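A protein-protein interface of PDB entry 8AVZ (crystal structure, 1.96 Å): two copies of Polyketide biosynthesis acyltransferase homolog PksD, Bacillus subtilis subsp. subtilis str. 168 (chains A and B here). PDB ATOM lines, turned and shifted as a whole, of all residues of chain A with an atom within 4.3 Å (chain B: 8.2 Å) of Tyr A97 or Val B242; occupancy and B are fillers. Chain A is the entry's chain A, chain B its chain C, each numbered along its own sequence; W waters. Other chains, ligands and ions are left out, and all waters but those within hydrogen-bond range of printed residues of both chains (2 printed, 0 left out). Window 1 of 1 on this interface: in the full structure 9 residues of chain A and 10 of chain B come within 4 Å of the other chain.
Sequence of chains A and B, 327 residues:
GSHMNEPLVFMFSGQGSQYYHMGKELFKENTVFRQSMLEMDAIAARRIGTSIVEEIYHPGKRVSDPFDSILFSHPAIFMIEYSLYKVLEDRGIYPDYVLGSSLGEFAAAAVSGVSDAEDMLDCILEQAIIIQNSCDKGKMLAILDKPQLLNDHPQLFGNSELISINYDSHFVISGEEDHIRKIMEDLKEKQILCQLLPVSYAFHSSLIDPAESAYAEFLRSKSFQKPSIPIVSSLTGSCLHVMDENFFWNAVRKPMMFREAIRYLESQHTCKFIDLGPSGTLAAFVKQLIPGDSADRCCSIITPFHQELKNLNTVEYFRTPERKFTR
The side-chain carboxylate of Asp A96 is in salt-bridge range of the side-chain amino group of Lys B226 (2.9 Å).
The backbone carbonyl oxygen (O) of Tyr A97 sits at hydrogen-bond distance from the backbone NH (N) of Phe A10, 3.0 Å away.
The backbone NH (N) of Val A98 lies within hydrogen-bond range of the backbone carbonyl oxygen (O) of Pro A230 (2.9 Å).
O of Leu A8 sits at hydrogen-bond distance from N of Tyr A97 (3.1 Å).
NE2 of His A269 is in hydrogen-bond range of OH of Tyr A97 (2.9 Å).
The side-chain carboxylate (OD2) of Asp A96 sits at hydrogen-bond distance from the backbone NH (N) of Leu A8, 2.8 Å away.
Val B242 touches Tyr A97 (N to OH, 3.97 Å).
CG of Pro A230 touches CG of His B241, at 3.5 Å.
Of the printed residues of chain B, Tyr A97 touches Val B242 (3.97 Å).
Of the printed residues of chain A, Lys B226 touches Asp A96 (2.9 Å).
Cys B239 touches none of the printed residues of chain A.
Printed residues of chain A within 4 Å of His B241: Pro A230.
Of chain A, only Tyr A97 comes within 4 Å of Val B242.
The nearest printed residue of chain B that does not touch Tyr A97 is His B241 (4.01 Å).
Of the 12 printed residues of chain A, 3 touch a printed residue of chain B.
Printed residues of chain A that touch a printed residue of chain B: Asp A96, Tyr A97 and Pro A230.
Hydrophobic or aromatic side chains of chain A that line the printed part of chain B: Tyr A97 and Pro A230.
Hydrophobic or aromatic side chains of chain B within 4 Å of the printed part of chain A: His B241.
Among the printed residues, 3 pairs touch across the chains.
Among the printed residues, Asp or Glu carboxylates within 4 Å of a Lys or Arg side-chain nitrogen of the other chain: Asp A96 with Lys B226.
No position is printed for both chains.
Of the 3 pairs that touch across the chains among the printed residues, none has its exchanged pair printed and touching as well.
Water W1 lies within hydrogen-bond range of the side-chain hydroxyl of Tyr A97 (2.5 Å), the backbone NH of His B241 (2.6 Å) and the backbone NH of Val B242 (3.3 Å).
Water W2 bridges the backbone carbonyl oxygen of Asp A96 (2.9 Å) and the side-chain amino group of Lys B226 (3.0 Å).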
ATOM      1  N   PRO A   7       4.742  14.037   5.211  1.00  0.00           N
ATOM      2  CA  PRO A   7       6.170  13.752   4.975  1.00  0.00           C
ATOM      3  C   PRO A   7       6.440  13.051   3.642  1.00  0.00           C
ATOM      4  O   PRO A   7       5.632  12.260   3.143  1.00  0.00           O
ATOM      5  CB  PRO A   7       6.564  12.850   6.147  1.00  0.00           C
ATOM      6  CG  PRO A   7       5.250  12.335   6.730  1.00  0.00           C
ATOM      7  CD  PRO A   7       4.149  13.254   6.315  1.00  0.00           C
ATOM      8  N   LEU A   8       7.623  13.334   3.093  1.00  0.00           N
ATOM      9  CA  LEU A   8       8.080  12.781   1.817  1.00  0.00           C
ATOM     10  C   LEU A   8       8.858  11.498   2.025  1.00  0.00           C
ATOM     11  O   LEU A   8       9.834  11.474   2.790  1.00  0.00           O
ATOM     12  CB  LEU A   8       8.993  13.750   1.068  1.00  0.00           C
ATOM     13  CG  LEU A   8       8.523  15.137   0.689  1.00  0.00           C
ATOM     14  CD1 LEU A   8       9.419  15.739  -0.437  1.00  0.00           C
ATOM     15  CD2 LEU A   8       7.183  14.911   0.157  1.00  0.00           C
ATOM     16  N   VAL A   9       8.474  10.466   1.277  1.00  0.00           N
ATOM     17  CA  VAL A   9       9.152   9.178   1.280  1.00  0.00           C
ATOM     18  C   VAL A   9       9.794   8.973  -0.095  1.00  0.00           C
ATOM     19  O   VAL A   9       9.094   8.957  -1.121  1.00  0.00           O
ATOM     20  CB  VAL A   9       8.177   8.043   1.628  1.00  0.00           C
ATOM     21  CG1 VAL A   9       8.924   6.660   1.653  1.00  0.00           C
ATOM     22  CG2 VAL A   9       7.551   8.315   3.010  1.00  0.00           C
ATOM     23  N   PHE A  10      11.118   8.820  -0.105  1.00  0.00           N
ATOM     24  CA  PHE A  10      11.869   8.484  -1.320  1.00  0.00           C
ATOM     25  C   PHE A  10      12.001   6.973  -1.366  1.00  0.00           C
ATOM     26  O   PHE A  10      12.494   6.358  -0.409  1.00  0.00           O
ATOM     27  CB  PHE A  10      13.274   9.110  -1.330  1.00  0.00           C
ATOM     28  CG  PHE A  10      13.331  10.587  -1.638  1.00  0.00           C
ATOM     29  CD1 PHE A  10      12.201  11.403  -1.593  1.00  0.00           C
ATOM     30  CD2 PHE A  10      14.568  11.173  -1.961  1.00  0.00           C
ATOM     31  CE1 PHE A  10      12.313  12.788  -1.850  1.00  0.00           C
ATOM     32  CE2 PHE A  10      14.676  12.533  -2.209  1.00  0.00           C
ATOM     33  CZ  PHE A  10      13.558  13.345  -2.165  1.00  0.00           C
ATOM     34  N   PRO A  95      14.100  14.038   1.525  1.00  0.00           N
ATOM     35  CA  PRO A  95      13.232  12.977   2.066  1.00  0.00           C
ATOM     36  C   PRO A  95      13.075  13.097   3.579  1.00  0.00           C
ATOM     37  O   PRO A  95      14.036  13.353   4.298  1.00  0.00           O
ATOM     38  CB  PRO A  95      13.988  11.695   1.701  1.00  0.00           C
ATOM     39  CG  PRO A  95      15.412  12.074   1.658  1.00  0.00           C
ATOM     40  CD  PRO A  95      15.474  13.561   1.245  1.00  0.00           C
ATOM     41  N   ASP A  96      11.856  12.886   4.076  1.00  0.00           N
ATOM     42  CA  ASP A  96      11.712  12.599   5.506  1.00  0.00           C
ATOM     43  C   ASP A  96      12.041  11.157   5.844  1.00  0.00           C
ATOM     44  O   ASP A  96      12.505  10.870   6.951  1.00  0.00           O
ATOM     45  CB  ASP A  96      10.303  12.912   5.956  1.00  0.00           C
ATOM     46  CG  ASP A  96       9.994  14.370   5.791  1.00  0.00           C
ATOM     47  OD1 ASP A  96      10.537  15.158   6.602  1.00  0.00           O
ATOM     48  OD2 ASP A  96       9.259  14.721   4.837  1.00  0.00           O
ATOM     49  N   TYR A  97      11.783  10.240   4.917  1.00  0.00           N
ATOM     50  CA  TYR A  97      12.089   8.832   5.084  1.00  0.00           C
ATOM     51  C   TYR A  97      12.629   8.348   3.753  1.00  0.00           C
ATOM     52  O   TYR A  97      12.209   8.841   2.712  1.00  0.00           O
ATOM     53  CB  TYR A  97      10.831   7.991   5.398  1.00  0.00           C
ATOM     54  CG  TYR A  97      10.108   8.336   6.672  1.00  0.00           C
ATOM     55  CD1 TYR A  97       9.102   9.314   6.683  1.00  0.00           C
ATOM     56  CD2 TYR A  97      10.374   7.644   7.843  1.00  0.00           C
ATOM     57  CE1 TYR A  97       8.412   9.617   7.841  1.00  0.00           C
ATOM     58  CE2 TYR A  97       9.705   7.965   9.027  1.00  0.00           C
ATOM     59  CZ  TYR A  97       8.718   8.940   9.003  1.00  0.00           C
ATOM     60  OH  TYR A  97       8.021   9.246  10.153  1.00  0.00           O
ATOM     61  N   VAL A  98      13.522   7.363   3.785  1.00  0.00           N
ATOM     62  CA  VAL A  98      13.861   6.626   2.585  1.00  0.00           C
ATOM     63  C   VAL A  98      13.367   5.201   2.775  1.00  0.00           C
ATOM     64  O   VAL A  98      13.333   4.678   3.891  1.00  0.00           O
ATOM     65  CB  VAL A  98      15.372   6.660   2.265  1.00  0.00           C
ATOM     66  CG1 VAL A  98      15.778   8.092   1.875  1.00  0.00           C
ATOM     67  CG2 VAL A  98      16.196   6.106   3.401  1.00  0.00           C
ATOM     68  N   PRO A 230      15.735   8.597   8.430  1.00  0.00           N
ATOM     69  CA  PRO A 230      15.040   7.348   8.783  1.00  0.00           C
ATOM     70  C   PRO A 230      14.920   6.434   7.577  1.00  0.00           C
ATOM     71  O   PRO A 230      14.412   6.863   6.537  1.00  0.00           O
ATOM     72  CB  PRO A 230      13.657   7.824   9.246  1.00  0.00           C
ATOM     73  CG  PRO A 230      13.803   9.252   9.597  1.00  0.00           C
ATOM     74  CD  PRO A 230      14.951   9.804   8.775  1.00  0.00           C
ATOM     75  N   VAL A 232      13.099   3.081   6.265  1.00  0.00           N
ATOM     76  CA  VAL A 232      12.097   2.030   6.398  1.00  0.00           C
ATOM     77  C   VAL A 232      12.500   0.933   5.417  1.00  0.00           C
ATOM     78  O   VAL A 232      12.689   1.193   4.225  1.00  0.00           O
ATOM     79  CB  VAL A 232      10.679   2.549   6.109  1.00  0.00           C
ATOM     80  CG1 VAL A 232       9.648   1.387   6.099  1.00  0.00           C
ATOM     81  CG2 VAL A 232      10.252   3.598   7.137  1.00  0.00           C
ATOM     82  N   LEU A 265       4.297   3.035   7.294  1.00  0.00           N
ATOM     83  CA  LEU A 265       4.390   4.472   7.054  1.00  0.00           C
ATOM     84  C   LEU A 265       3.019   5.136   7.080  1.00  0.00           C
ATOM     85  O   LEU A 265       2.875   6.261   7.578  1.00  0.00           O
ATOM     86  CB  LEU A 265       5.095   4.745   5.720  1.00  0.00           C
ATOM     87  CG  LEU A 265       6.613   4.610   5.759  1.00  0.00           C
ATOM     88  CD1 LEU A 265       7.133   4.536   4.345  1.00  0.00           C
ATOM     89  CD2 LEU A 265       7.271   5.837   6.499  1.00  0.00           C
ATOM     90  N   HIS A 269       1.260   8.501   9.463  1.00  0.00           N
ATOM     91  CA  HIS A 269       0.812   9.744   8.832  1.00  0.00           C
ATOM     92  C   HIS A 269       0.519   9.464   7.369  1.00  0.00           C
ATOM     93  O   HIS A 269       0.859   8.403   6.842  1.00  0.00           O
ATOM     94  CB  HIS A 269       1.827  10.885   8.997  1.00  0.00           C
ATOM     95  CG  HIS A 269       3.234  10.401   9.055  1.00  0.00           C
ATOM     96  ND1 HIS A 269       3.806   9.668   8.039  1.00  0.00           N
ATOM     97  CD2 HIS A 269       4.190  10.549  10.005  1.00  0.00           C
ATOM     98  CE1 HIS A 269       5.045   9.354   8.377  1.00  0.00           C
ATOM     99  NE2 HIS A 269       5.304   9.877   9.563  1.00  0.00           N
ATOM    100  N   GLN B 225      10.471  22.368  16.434  1.00  0.00           N
ATOM    101  CA  GLN B 225      11.556  21.881  15.604  1.00  0.00           C
ATOM    102  C   GLN B 225      11.402  20.388  15.339  1.00  0.00           C
ATOM    103  O   GLN B 225      10.606  19.689  15.974  1.00  0.00           O
ATOM    104  CB  GLN B 225      12.893  22.162  16.286  1.00  0.00           C
ATOM    105  CG  GLN B 225      13.113  23.636  16.537  1.00  0.00           C
ATOM    106  CD  GLN B 225      13.124  24.427  15.255  1.00  0.00           C
ATOM    107  OE1 GLN B 225      13.839  24.080  14.311  1.00  0.00           O
ATOM    108  NE2 GLN B 225      12.306  25.481  15.197  1.00  0.00           N
ATOM    109  N   LYS B 226      12.185  19.897  14.407  1.00  0.00           N
ATOM    110  CA  LYS B 226      12.210  18.467  14.200  1.00  0.00           C
ATOM    111  C   LYS B 226      12.965  17.820  15.362  1.00  0.00           C
ATOM    112  O   LYS B 226      13.830  18.447  15.968  1.00  0.00           O
ATOM    113  CB  LYS B 226      12.892  18.126  12.864  1.00  0.00           C
ATOM    114  CG  LYS B 226      11.893  17.785  11.735  1.00  0.00           C
ATOM    115  CD  LYS B 226      11.584  16.268  11.598  1.00  0.00           C
ATOM    116  CE  LYS B 226      10.944  15.887  10.245  1.00  0.00           C
ATOM    117  NZ  LYS B 226      11.872  15.409   9.128  1.00  0.00           N
ATOM    118  N   PRO B 227      12.643  16.585  15.724  1.00  0.00           N
ATOM    119  CA  PRO B 227      13.472  15.888  16.708  1.00  0.00           C
ATOM    120  C   PRO B 227      14.932  15.934  16.302  1.00  0.00           C
ATOM    121  O   PRO B 227      15.287  15.726  15.139  1.00  0.00           O
ATOM    122  CB  PRO B 227      12.925  14.457  16.683  1.00  0.00           C
ATOM    123  CG  PRO B 227      11.523  14.629  16.282  1.00  0.00           C
ATOM    124  CD  PRO B 227      11.529  15.747  15.268  1.00  0.00           C
ATOM    125  N   ILE B 231      13.469  10.012  19.229  1.00  0.00           N
ATOM    126  CA  ILE B 231      12.330   9.906  20.128  1.00  0.00           C
ATOM    127  C   ILE B 231      11.653   8.570  19.878  1.00  0.00           C
ATOM    128  O   ILE B 231      11.419   8.185  18.723  1.00  0.00           O
ATOM    129  CB  ILE B 231      11.324  11.049  19.911  1.00  0.00           C
ATOM    130  CG1 ILE B 231      11.954  12.397  20.217  1.00  0.00           C
ATOM    131  CG2 ILE B 231      10.059  10.834  20.784  1.00  0.00           C
ATOM    132  CD1 ILE B 231      11.009  13.557  19.966  1.00  0.00           C
ATOM    133  N   THR B 236       2.546   6.722  19.923  1.00  0.00           N
ATOM    134  CA  THR B 236       2.563   6.015  18.638  1.00  0.00           C
ATOM    135  C   THR B 236       3.024   4.564  18.728  1.00  0.00           C
ATOM    136  O   THR B 236       2.870   3.825  17.752  1.00  0.00           O
ATOM    137  CB  THR B 236       3.472   6.758  17.643  1.00  0.00           C
ATOM    138  OG1 THR B 236       4.828   6.575  18.048  1.00  0.00           O
ATOM    139  CG2 THR B 236       3.165   8.247  17.638  1.00  0.00           C
ATOM    140  N   CYS B 239       9.276   4.520  17.029  1.00  0.00           N
ATOM    141  CA  CYS B 239      10.107   5.682  16.827  1.00  0.00           C
ATOM    142  C   CYS B 239       9.272   6.805  16.251  1.00  0.00           C
ATOM    143  O   CYS B 239       8.233   6.589  15.632  1.00  0.00           O
ATOM    144  CB  CYS B 239      11.324   5.296  15.954  1.00  0.00           C
ATOM    145  SG  CYS B 239      10.738   4.596  14.368  1.00  0.00           S
ATOM    146  N   LEU B 240       9.674   8.022  16.557  1.00  0.00           N
ATOM    147  CA  LEU B 240       8.903   9.169  16.125  1.00  0.00           C
ATOM    148  C   LEU B 240       9.881  10.107  15.423  1.00  0.00           C
ATOM    149  O   LEU B 240      10.757  10.706  16.062  1.00  0.00           O
ATOM    150  CB  LEU B 240       8.201   9.828  17.314  1.00  0.00           C
ATOM    151  CG  LEU B 240       7.254  10.889  16.777  1.00  0.00           C
ATOM    152  CD1 LEU B 240       5.945  10.842  17.466  1.00  0.00           C
ATOM    153  CD2 LEU B 240       7.907  12.217  16.936  1.00  0.00           C
ATOM    154  N   HIS B 241       9.771  10.197  14.105  1.00  0.00           N
ATOM    155  CA  HIS B 241      10.664  11.077  13.365  1.00  0.00           C
ATOM    156  C   HIS B 241       9.995  12.326  12.874  1.00  0.00           C
ATOM    157  O   HIS B 241      10.647  13.345  12.767  1.00  0.00           O
ATOM    158  CB  HIS B 241      11.301  10.339  12.179  1.00  0.00           C
ATOM    159  CG  HIS B 241      12.008   9.095  12.597  1.00  0.00           C
ATOM    160  ND1 HIS B 241      13.253   9.141  13.182  1.00  0.00           N
ATOM    161  CD2 HIS B 241      11.645   7.789  12.570  1.00  0.00           C
ATOM    162  CE1 HIS B 241      13.645   7.914  13.472  1.00  0.00           C
ATOM    163  NE2 HIS B 241      12.691   7.077  13.110  1.00  0.00           N
ATOM    164  N   VAL B 242       8.705  12.274  12.633  1.00  0.00           N
ATOM    165  CA  VAL B 242       7.950  13.397  12.123  1.00  0.00           C
ATOM    166  C   VAL B 242       6.719  13.529  12.996  1.00  0.00           C
ATOM    167  O   VAL B 242       5.965  12.565  13.173  1.00  0.00           O
ATOM    168  CB  VAL B 242       7.551  13.205  10.649  1.00  0.00           C
ATOM    169  CG1 VAL B 242       6.612  14.316  10.224  1.00  0.00           C
ATOM    170  CG2 VAL B 242       8.813  13.170   9.765  1.00  0.00           C
ATOM    171  N   MET B 243       6.512  14.722  13.514  1.00  0.00           N
ATOM    172  CA  MET B 243       5.493  14.989  14.497  1.00  0.00           C
ATOM    173  C   MET B 243       4.303  15.666  13.810  1.00  0.00           C
ATOM    174  O   MET B 243       4.521  16.606  13.058  1.00  0.00           O
ATOM    175  CB  MET B 243       6.114  15.889  15.550  1.00  0.00           C
ATOM    176  CG  MET B 243       5.293  16.119  16.727  1.00  0.00           C
ATOM    177  SD  MET B 243       6.460  16.544  18.231  1.00  0.00           S
ATOM    178  CE  MET B 243       7.932  15.353  18.083  1.00  0.00           C
ATOM    179  N   ASP B 244       3.065  15.210  14.012  1.00  0.00           N
ATOM    180  CA  ASP B 244       1.959  15.972  13.436  1.00  0.00           C
ATOM    181  C   ASP B 244       1.542  17.150  14.348  1.00  0.00           C
ATOM    182  O   ASP B 244       2.106  17.389  15.423  1.00  0.00           O
ATOM    183  CB  ASP B 244       0.786  15.048  13.069  1.00  0.00           C
ATOM    184  CG  ASP B 244      -0.062  14.615  14.268  1.00  0.00           C
ATOM    185  OD1 ASP B 244       0.087  15.144  15.388  1.00  0.00           O
ATOM    186  OD2 ASP B 244      -0.911  13.719  14.081  1.00  0.00           O
ATOM    187  N   GLU B 245       0.526  17.893  13.890  1.00  0.00           N
ATOM    188  CA  GLU B 245       0.129  19.152  14.524  1.00  0.00           C
ATOM    189  C   GLU B 245      -0.358  18.937  15.953  1.00  0.00           C
ATOM    190  O   GLU B 245      -0.113  19.768  16.836  1.00  0.00           O
ATOM    191  CB  GLU B 245      -0.989  19.792  13.702  1.00  0.00           C
ATOM    192  CG  GLU B 245      -0.775  21.211  13.222  1.00  0.00           C
ATOM    193  CD  GLU B 245      -1.973  21.705  12.409  1.00  0.00           C
ATOM    194  OE1 GLU B 245      -2.808  20.853  12.003  1.00  0.00           O
ATOM    195  OE2 GLU B 245      -2.098  22.938  12.205  1.00  0.00           O
ATOM    196  N   PHE B 247       0.283  16.506  18.153  1.00  0.00           N
ATOM    197  CA  PHE B 247       1.054  15.631  19.024  1.00  0.00           C
ATOM    198  C   PHE B 247       0.898  15.998  20.500  1.00  0.00           C
ATOM    199  O   PHE B 247       0.680  15.124  21.339  1.00  0.00           O
ATOM    200  CB  PHE B 247       2.519  15.647  18.643  1.00  0.00           C
ATOM    201  CG  PHE B 247       3.368  14.825  19.560  1.00  0.00           C
ATOM    202  CD1 PHE B 247       3.396  13.452  19.446  1.00  0.00           C
ATOM    203  CD2 PHE B 247       4.149  15.424  20.527  1.00  0.00           C
ATOM    204  CE1 PHE B 247       4.181  12.686  20.286  1.00  0.00           C
ATOM    205  CE2 PHE B 247       4.937  14.669  21.375  1.00  0.00           C
ATOM    206  CZ  PHE B 247       4.948  13.286  21.252  1.00  0.00           C
HETATM  207  O   HOH W   1       7.878   9.082  12.685  1.00  0.00           O
HETATM  208  O   HOH W   2      12.969  12.590   9.211  1.00  0.00           O
